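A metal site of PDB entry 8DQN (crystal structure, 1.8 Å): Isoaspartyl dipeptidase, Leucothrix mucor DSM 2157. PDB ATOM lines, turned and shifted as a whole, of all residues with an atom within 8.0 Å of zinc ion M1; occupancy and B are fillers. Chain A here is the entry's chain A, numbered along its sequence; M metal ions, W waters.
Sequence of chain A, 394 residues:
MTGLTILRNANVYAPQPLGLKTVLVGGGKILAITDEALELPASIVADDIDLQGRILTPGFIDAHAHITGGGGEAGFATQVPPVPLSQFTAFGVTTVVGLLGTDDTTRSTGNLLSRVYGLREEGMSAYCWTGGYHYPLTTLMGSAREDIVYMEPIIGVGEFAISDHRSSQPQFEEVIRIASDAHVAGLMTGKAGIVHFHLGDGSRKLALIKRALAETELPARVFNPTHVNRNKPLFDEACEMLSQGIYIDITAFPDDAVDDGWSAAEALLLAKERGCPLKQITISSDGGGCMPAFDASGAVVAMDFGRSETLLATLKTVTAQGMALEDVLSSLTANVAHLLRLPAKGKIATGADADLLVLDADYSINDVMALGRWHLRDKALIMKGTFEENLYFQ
The side-chain carboxylate of Glu 159 lies close to a ring nitrogen (NE2) of His 64 (3.3 Å).
NE2 of His 198 is in hydrogen-bond range of OD2 of Asp 164, at 2.8 Å.
N of His 198 lies within hydrogen-bond range of O of Phe 160.
NE2 of His 198 lies within hydrogen-bond range of OH of Tyr 133.
ND1 of His 227 sits at hydrogen-bond distance from OG1 of Thr 251 (2.7 Å).
A ring nitrogen (ND1) of His 198 is bound to zinc ion M1, at 2.1 Å.
NE2 of His 227 binds zinc ion M1 (2.3 Å).
Zinc ion M1 is bound by the side-chain carboxylate (OE1) of Glu 159.
The nearest printed residue that does not touch zinc ion M1 is His 64 (4.2 Å).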
ATOM      1  N   HIS A  64     -19.413 -18.136 -15.081  1.00  0.00           N
ATOM      2  CA  HIS A  64     -19.006 -18.445 -13.690  1.00  0.00           C
ATOM      3  C   HIS A  64     -18.122 -17.304 -13.184  1.00  0.00           C
ATOM      4  O   HIS A  64     -16.909 -17.394 -13.336  1.00  0.00           O
ATOM      5  CB  HIS A  64     -18.276 -19.799 -13.623  1.00  0.00           C
ATOM      6  CG  HIS A  64     -18.018 -20.297 -12.255  1.00  0.00           C
ATOM      7  ND1 HIS A  64     -18.576 -21.489 -11.804  1.00  0.00           N
ATOM      8  CD2 HIS A  64     -17.281 -19.792 -11.241  1.00  0.00           C
ATOM      9  CE1 HIS A  64     -18.191 -21.694 -10.553  1.00  0.00           C
ATOM     10  NE2 HIS A  64     -17.368 -20.683 -10.181  1.00  0.00           N
ATOM     11  N   HIS A  66     -17.743 -14.369  -9.812  1.00  0.00           N
ATOM     12  CA  HIS A  66     -18.125 -13.747  -8.531  1.00  0.00           C
ATOM     13  C   HIS A  66     -18.187 -12.244  -8.735  1.00  0.00           C
ATOM     14  O   HIS A  66     -17.269 -11.563  -8.320  1.00  0.00           O
ATOM     15  CB  HIS A  66     -17.132 -14.126  -7.428  1.00  0.00           C
ATOM     16  CG  HIS A  66     -17.095 -15.578  -7.197  1.00  0.00           C
ATOM     17  ND1 HIS A  66     -17.967 -16.182  -6.309  1.00  0.00           N
ATOM     18  CD2 HIS A  66     -16.351 -16.558  -7.746  1.00  0.00           C
ATOM     19  CE1 HIS A  66     -17.729 -17.480  -6.298  1.00  0.00           C
ATOM     20  NE2 HIS A  66     -16.740 -17.735  -7.169  1.00  0.00           N
ATOM     21  N   GLU A  73     -13.386 -17.410   2.620  1.00  0.00           N
ATOM     22  CA  GLU A  73     -13.213 -18.844   2.974  1.00  0.00           C
ATOM     23  C   GLU A  73     -12.067 -19.032   3.973  1.00  0.00           C
ATOM     24  O   GLU A  73     -11.968 -20.126   4.486  1.00  0.00           O
ATOM     25  CB  GLU A  73     -12.724 -19.700   1.809  1.00  0.00           C
ATOM     26  CG  GLU A  73     -13.629 -19.717   0.641  1.00  0.00           C
ATOM     27  CD  GLU A  73     -13.409 -20.992  -0.180  1.00  0.00           C
ATOM     28  OE1 GLU A  73     -12.780 -21.987   0.354  1.00  0.00           O
ATOM     29  OE2 GLU A  73     -13.901 -21.006  -1.337  1.00  0.00           O
ATOM     30  N   LEU A  99     -22.460 -15.477  -9.525  1.00  0.00           N
ATOM     31  CA  LEU A  99     -22.875 -16.468  -8.512  1.00  0.00           C
ATOM     32  C   LEU A  99     -22.189 -16.142  -7.187  1.00  0.00           C
ATOM     33  O   LEU A  99     -21.193 -15.406  -7.170  1.00  0.00           O
ATOM     34  CB  LEU A  99     -22.562 -17.903  -8.954  1.00  0.00           C
ATOM     35  CG  LEU A  99     -21.276 -18.134  -9.760  1.00  0.00           C
ATOM     36  CD1 LEU A  99     -20.041 -17.884  -8.920  1.00  0.00           C
ATOM     37  CD2 LEU A  99     -21.225 -19.543 -10.303  1.00  0.00           C
ATOM     38  N   LEU A 100     -22.802 -16.629  -6.116  1.00  0.00           N
ATOM     39  CA  LEU A 100     -22.170 -16.765  -4.787  1.00  0.00           C
ATOM     40  C   LEU A 100     -21.480 -18.137  -4.747  1.00  0.00           C
ATOM     41  O   LEU A 100     -22.010 -19.146  -5.345  1.00  0.00           O
ATOM     42  CB  LEU A 100     -23.262 -16.683  -3.721  1.00  0.00           C
ATOM     43  CG  LEU A 100     -24.106 -15.417  -3.724  1.00  0.00           C
ATOM     44  CD1 LEU A 100     -25.022 -15.424  -2.528  1.00  0.00           C
ATOM     45  CD2 LEU A 100     -23.229 -14.165  -3.711  1.00  0.00           C
ATOM     46  N   GLY A 101     -20.370 -18.174  -4.043  1.00  0.00           N
ATOM     47  CA  GLY A 101     -19.619 -19.413  -3.763  1.00  0.00           C
ATOM     48  C   GLY A 101     -19.707 -19.768  -2.288  1.00  0.00           C
ATOM     49  O   GLY A 101     -20.800 -19.743  -1.710  1.00  0.00           O
ATOM     50  N   THR A 102     -18.561 -20.103  -1.690  1.00  0.00           N
ATOM     51  CA  THR A 102     -18.488 -20.701  -0.355  1.00  0.00           C
ATOM     52  C   THR A 102     -19.175 -19.767   0.641  1.00  0.00           C
ATOM     53  O   THR A 102     -19.886 -20.276   1.502  1.00  0.00           O
ATOM     54  CB  THR A 102     -17.051 -20.991   0.066  1.00  0.00           C
ATOM     55  OG1 THR A 102     -16.482 -21.689  -1.028  1.00  0.00           O
ATOM     56  CG2 THR A 102     -16.995 -21.769   1.367  1.00  0.00           C
ATOM     57  N   TYR A 133     -24.088 -22.251  -2.727  1.00  0.00           N
ATOM     58  CA  TYR A 133     -23.160 -23.388  -2.546  1.00  0.00           C
ATOM     59  C   TYR A 133     -23.716 -24.433  -1.576  1.00  0.00           C
ATOM     60  O   TYR A 133     -23.522 -25.633  -1.764  1.00  0.00           O
ATOM     61  CB  TYR A 133     -21.924 -22.721  -2.009  1.00  0.00           C
ATOM     62  CG  TYR A 133     -20.628 -23.466  -2.152  1.00  0.00           C
ATOM     63  CD1 TYR A 133     -20.202 -24.275  -1.119  1.00  0.00           C
ATOM     64  CD2 TYR A 133     -19.753 -23.184  -3.182  1.00  0.00           C
ATOM     65  CE1 TYR A 133     -18.954 -24.876  -1.144  1.00  0.00           C
ATOM     66  CE2 TYR A 133     -18.493 -23.759  -3.216  1.00  0.00           C
ATOM     67  CZ  TYR A 133     -18.096 -24.598  -2.184  1.00  0.00           C
ATOM     68  OH  TYR A 133     -16.886 -25.238  -2.172  1.00  0.00           O
ATOM     69  N   GLU A 159     -23.527 -21.653  -7.417  1.00  0.00           N
ATOM     70  CA  GLU A 159     -22.845 -22.878  -7.777  1.00  0.00           C
ATOM     71  C   GLU A 159     -22.957 -23.869  -6.622  1.00  0.00           C
ATOM     72  O   GLU A 159     -22.397 -23.616  -5.561  1.00  0.00           O
ATOM     73  CB  GLU A 159     -21.370 -22.649  -8.086  1.00  0.00           C
ATOM     74  CG  GLU A 159     -20.693 -21.843  -7.025  1.00  0.00           C
ATOM     75  CD  GLU A 159     -19.177 -21.865  -7.118  1.00  0.00           C
ATOM     76  OE1 GLU A 159     -18.668 -22.695  -7.877  1.00  0.00           O
ATOM     77  OE2 GLU A 159     -18.552 -21.022  -6.446  1.00  0.00           O
ATOM     78  N   PHE A 160     -23.724 -24.922  -6.792  1.00  0.00           N
ATOM     79  CA  PHE A 160     -24.129 -25.821  -5.685  1.00  0.00           C
ATOM     80  C   PHE A 160     -23.052 -26.889  -5.521  1.00  0.00           C
ATOM     81  O   PHE A 160     -22.731 -27.551  -6.518  1.00  0.00           O
ATOM     82  CB  PHE A 160     -25.481 -26.438  -5.994  1.00  0.00           C
ATOM     83  CG  PHE A 160     -26.033 -27.209  -4.836  1.00  0.00           C
ATOM     84  CD1 PHE A 160     -26.478 -26.546  -3.703  1.00  0.00           C
ATOM     85  CD2 PHE A 160     -26.066 -28.593  -4.851  1.00  0.00           C
ATOM     86  CE1 PHE A 160     -26.946 -27.238  -2.616  1.00  0.00           C
ATOM     87  CE2 PHE A 160     -26.547 -29.289  -3.761  1.00  0.00           C
ATOM     88  CZ  PHE A 160     -26.980 -28.618  -2.653  1.00  0.00           C
ATOM     89  N   ALA A 161     -22.500 -27.044  -4.333  1.00  0.00           N
ATOM     90  CA  ALA A 161     -21.270 -27.843  -4.118  1.00  0.00           C
ATOM     91  C   ALA A 161     -21.619 -29.311  -3.900  1.00  0.00           C
ATOM     92  O   ALA A 161     -22.483 -29.636  -3.078  1.00  0.00           O
ATOM     93  CB  ALA A 161     -20.516 -27.274  -2.969  1.00  0.00           C
ATOM     94  N   ASP A 164     -17.092 -32.190  -2.091  1.00  0.00           N
ATOM     95  CA  ASP A 164     -16.203 -31.136  -1.564  1.00  0.00           C
ATOM     96  C   ASP A 164     -16.360 -31.041  -0.055  1.00  0.00           C
ATOM     97  O   ASP A 164     -17.505 -31.047   0.439  1.00  0.00           O
ATOM     98  CB  ASP A 164     -16.488 -29.783  -2.226  1.00  0.00           C
ATOM     99  CG  ASP A 164     -15.401 -28.745  -1.979  1.00  0.00           C
ATOM    100  OD1 ASP A 164     -15.297 -28.246  -0.856  1.00  0.00           O
ATOM    101  OD2 ASP A 164     -14.643 -28.452  -2.912  1.00  0.00           O
ATOM    102  N   ARG A 166     -16.243 -28.540   1.714  1.00  0.00           N
ATOM    103  CA  ARG A 166     -17.011 -27.306   2.057  1.00  0.00           C
ATOM    104  C   ARG A 166     -18.472 -27.440   1.656  1.00  0.00           C
ATOM    105  O   ARG A 166     -19.215 -26.491   1.868  1.00  0.00           O
ATOM    106  CB  ARG A 166     -16.386 -26.101   1.363  1.00  0.00           C
ATOM    107  CG  ARG A 166     -14.972 -25.815   1.838  1.00  0.00           C
ATOM    108  CD  ARG A 166     -14.174 -25.013   0.851  1.00  0.00           C
ATOM    109  NE  ARG A 166     -13.990 -25.765  -0.387  1.00  0.00           N
ATOM    110  CZ  ARG A 166     -13.334 -25.330  -1.453  1.00  0.00           C
ATOM    111  NH1 ARG A 166     -12.781 -24.122  -1.432  1.00  0.00           N
ATOM    112  NH2 ARG A 166     -13.245 -26.073  -2.548  1.00  0.00           N
ATOM    113  N   HIS A 196     -25.878 -25.511 -11.915  1.00  0.00           N
ATOM    114  CA  HIS A 196     -24.435 -25.331 -12.070  1.00  0.00           C
ATOM    115  C   HIS A 196     -23.783 -25.854 -10.791  1.00  0.00           C
ATOM    116  O   HIS A 196     -23.924 -25.211  -9.756  1.00  0.00           O
ATOM    117  CB  HIS A 196     -24.191 -23.865 -12.388  1.00  0.00           C
ATOM    118  CG  HIS A 196     -22.819 -23.539 -12.812  1.00  0.00           C
ATOM    119  ND1 HIS A 196     -22.343 -23.874 -14.065  1.00  0.00           N
ATOM    120  CD2 HIS A 196     -21.841 -22.816 -12.188  1.00  0.00           C
ATOM    121  CE1 HIS A 196     -21.105 -23.390 -14.186  1.00  0.00           C
ATOM    122  NE2 HIS A 196     -20.784 -22.758 -13.037  1.00  0.00           N
ATOM    123  N   PHE A 197     -23.115 -27.010 -10.864  1.00  0.00           N
ATOM    124  CA  PHE A 197     -22.534 -27.704  -9.691  1.00  0.00           C
ATOM    125  C   PHE A 197     -21.046 -27.391  -9.579  1.00  0.00           C
ATOM    126  O   PHE A 197     -20.322 -27.614 -10.528  1.00  0.00           O
ATOM    127  CB  PHE A 197     -22.668 -29.207  -9.797  1.00  0.00           C
ATOM    128  CG  PHE A 197     -24.060 -29.758  -9.671  1.00  0.00           C
ATOM    129  CD1 PHE A 197     -24.584 -30.072  -8.427  1.00  0.00           C
ATOM    130  CD2 PHE A 197     -24.824 -29.986 -10.792  1.00  0.00           C
ATOM    131  CE1 PHE A 197     -25.862 -30.595  -8.327  1.00  0.00           C
ATOM    132  CE2 PHE A 197     -26.092 -30.530 -10.682  1.00  0.00           C
ATOM    133  CZ  PHE A 197     -26.610 -30.828  -9.453  1.00  0.00           C
ATOM    134  N   HIS A 198     -20.619 -26.887  -8.431  1.00  0.00           N
ATOM    135  CA  HIS A 198     -19.200 -26.816  -8.037  1.00  0.00           C
ATOM    136  C   HIS A 198     -18.773 -28.236  -7.702  1.00  0.00           C
ATOM    137  O   HIS A 198     -19.419 -28.864  -6.836  1.00  0.00           O
ATOM    138  CB  HIS A 198     -18.985 -25.886  -6.841  1.00  0.00           C
ATOM    139  CG  HIS A 198     -17.726 -26.195  -6.084  1.00  0.00           C
ATOM    140  ND1 HIS A 198     -16.565 -25.486  -6.286  1.00  0.00           N
ATOM    141  CD2 HIS A 198     -17.412 -27.171  -5.187  1.00  0.00           C
ATOM    142  CE1 HIS A 198     -15.609 -25.962  -5.515  1.00  0.00           C
ATOM    143  NE2 HIS A 198     -16.110 -26.991  -4.829  1.00  0.00           N
ATOM    144  N   LEU A 199     -17.744 -28.742  -8.357  1.00  0.00           N
ATOM    145  CA  LEU A 199     -17.092 -30.027  -7.990  1.00  0.00           C
ATOM    146  C   LEU A 199     -15.854 -29.718  -7.175  1.00  0.00           C
ATOM    147  O   LEU A 199     -15.081 -28.803  -7.563  1.00  0.00           O
ATOM    148  CB  LEU A 199     -16.722 -30.829  -9.232  1.00  0.00           C
ATOM    149  CG  LEU A 199     -17.782 -31.817  -9.706  1.00  0.00           C
ATOM    150  CD1 LEU A 199     -17.926 -32.956  -8.711  1.00  0.00           C
ATOM    151  CD2 LEU A 199     -19.122 -31.124  -9.918  1.00  0.00           C
ATOM    152  N   GLY A 200     -15.669 -30.460  -6.090  1.00  0.00           N
ATOM    153  CA  GLY A 200     -14.398 -30.496  -5.362  1.00  0.00           C
ATOM    154  C   GLY A 200     -13.593 -31.729  -5.709  1.00  0.00           C
ATOM    155  O   GLY A 200     -13.922 -32.410  -6.727  1.00  0.00           O
ATOM    156  N   THR A 226     -19.027 -27.942 -13.073  1.00  0.00           N
ATOM    157  CA  THR A 226     -17.925 -27.010 -13.369  1.00  0.00           C
ATOM    158  C   THR A 226     -16.692 -27.461 -12.579  1.00  0.00           C
ATOM    159  O   THR A 226     -16.815 -28.369 -11.718  1.00  0.00           O
ATOM    160  CB  THR A 226     -18.317 -25.555 -13.102  1.00  0.00           C
ATOM    161  OG1 THR A 226     -17.281 -24.714 -13.639  1.00  0.00           O
ATOM    162  CG2 THR A 226     -18.438 -25.220 -11.633  1.00  0.00           C
ATOM    163  N   HIS A 227     -15.548 -26.855 -12.883  1.00  0.00           N
ATOM    164  CA  HIS A 227     -14.201 -27.236 -12.397  1.00  0.00           C
ATOM    165  C   HIS A 227     -13.889 -28.704 -12.663  1.00  0.00           C
ATOM    166  O   HIS A 227     -13.153 -29.291 -11.878  1.00  0.00           O
ATOM    167  CB  HIS A 227     -14.019 -27.008 -10.893  1.00  0.00           C
ATOM    168  CG  HIS A 227     -14.553 -25.722 -10.402  1.00  0.00           C
ATOM    169  ND1 HIS A 227     -14.213 -24.487 -10.914  1.00  0.00           N
ATOM    170  CD2 HIS A 227     -15.428 -25.520  -9.408  1.00  0.00           C
ATOM    171  CE1 HIS A 227     -14.854 -23.552 -10.245  1.00  0.00           C
ATOM    172  NE2 HIS A 227     -15.625 -24.178  -9.302  1.00  0.00           N
ATOM    173  N   ARG A 230     -10.254 -29.993 -12.493  1.00  0.00           N
ATOM    174  CA  ARG A 230      -9.448 -29.773 -11.260  1.00  0.00           C
ATOM    175  C   ARG A 230      -8.680 -31.030 -10.860  1.00  0.00           C
ATOM    176  O   ARG A 230      -7.713 -30.877 -10.153  1.00  0.00           O
ATOM    177  CB  ARG A 230     -10.327 -29.334 -10.071  1.00  0.00           C
ATOM    178  CG  ARG A 230     -11.349 -30.363  -9.637  1.00  0.00           C
ATOM    179  CD  ARG A 230     -12.265 -29.844  -8.533  1.00  0.00           C
ATOM    180  NE  ARG A 230     -11.438 -29.431  -7.400  1.00  0.00           N
ATOM    181  CZ  ARG A 230     -11.517 -28.269  -6.767  1.00  0.00           C
ATOM    182  NH1 ARG A 230     -12.439 -27.374  -7.063  1.00  0.00           N
ATOM    183  NH2 ARG A 230     -10.665 -28.040  -5.801  1.00  0.00           N
ATOM    184  N   THR A 251     -12.732 -24.834 -16.065  1.00  0.00           N
ATOM    185  CA  THR A 251     -12.346 -23.553 -15.449  1.00  0.00           C
ATOM    186  C   THR A 251     -10.960 -23.165 -15.960  1.00  0.00           C
ATOM    187  O   THR A 251     -10.034 -23.976 -15.822  1.00  0.00           O
ATOM    188  CB  THR A 251     -12.360 -23.653 -13.920  1.00  0.00           C
ATOM    189  OG1 THR A 251     -13.631 -24.173 -13.546  1.00  0.00           O
ATOM    190  CG2 THR A 251     -12.106 -22.322 -13.272  1.00  0.00           C
ATOM    191  N   PHE A 253      -8.441 -21.702 -14.703  1.00  0.00           N
ATOM    192  CA  PHE A 253      -7.588 -21.438 -13.525  1.00  0.00           C
ATOM    193  C   PHE A 253      -6.366 -20.655 -14.022  1.00  0.00           C
ATOM    194  O   PHE A 253      -5.847 -20.909 -15.132  1.00  0.00           O
ATOM    195  CB  PHE A 253      -7.051 -22.746 -12.931  1.00  0.00           C
ATOM    196  CG  PHE A 253      -8.042 -23.768 -12.433  1.00  0.00           C
ATOM    197  CD1 PHE A 253      -8.888 -23.429 -11.390  1.00  0.00           C
ATOM    198  CD2 PHE A 253      -8.070 -25.070 -12.933  1.00  0.00           C
ATOM    199  CE1 PHE A 253      -9.807 -24.345 -10.889  1.00  0.00           C
ATOM    200  CE2 PHE A 253      -8.974 -25.995 -12.416  1.00  0.00           C
ATOM    201  CZ  PHE A 253      -9.861 -25.618 -11.416  1.00  0.00           C
ATOM    202  N   ASP A 286     -13.971 -18.068 -13.476  1.00  0.00           N
ATOM    203  CA  ASP A 286     -14.060 -17.827 -12.011  1.00  0.00           C
ATOM    204  C   ASP A 286     -13.530 -16.430 -11.622  1.00  0.00           C
ATOM    205  O   ASP A 286     -12.920 -16.295 -10.529  1.00  0.00           O
ATOM    206  CB  ASP A 286     -13.342 -18.964 -11.257  1.00  0.00           C
ATOM    207  CG  ASP A 286     -13.765 -19.022  -9.805  1.00  0.00           C
ATOM    208  OD1 ASP A 286     -14.910 -18.576  -9.521  1.00  0.00           O
ATOM    209  OD2 ASP A 286     -12.918 -19.378  -8.944  1.00  0.00           O
HETATM  210 ZN    ZN M   1     -16.501 -23.556  -7.218  1.00  0.00          ZN
HETATM  211 ZN    ZN M   2     -16.071 -20.248  -7.571  1.00  0.00          ZN
HETATM  212  O   HOH W   1     -14.269 -21.834  -6.382  1.00  0.00           O
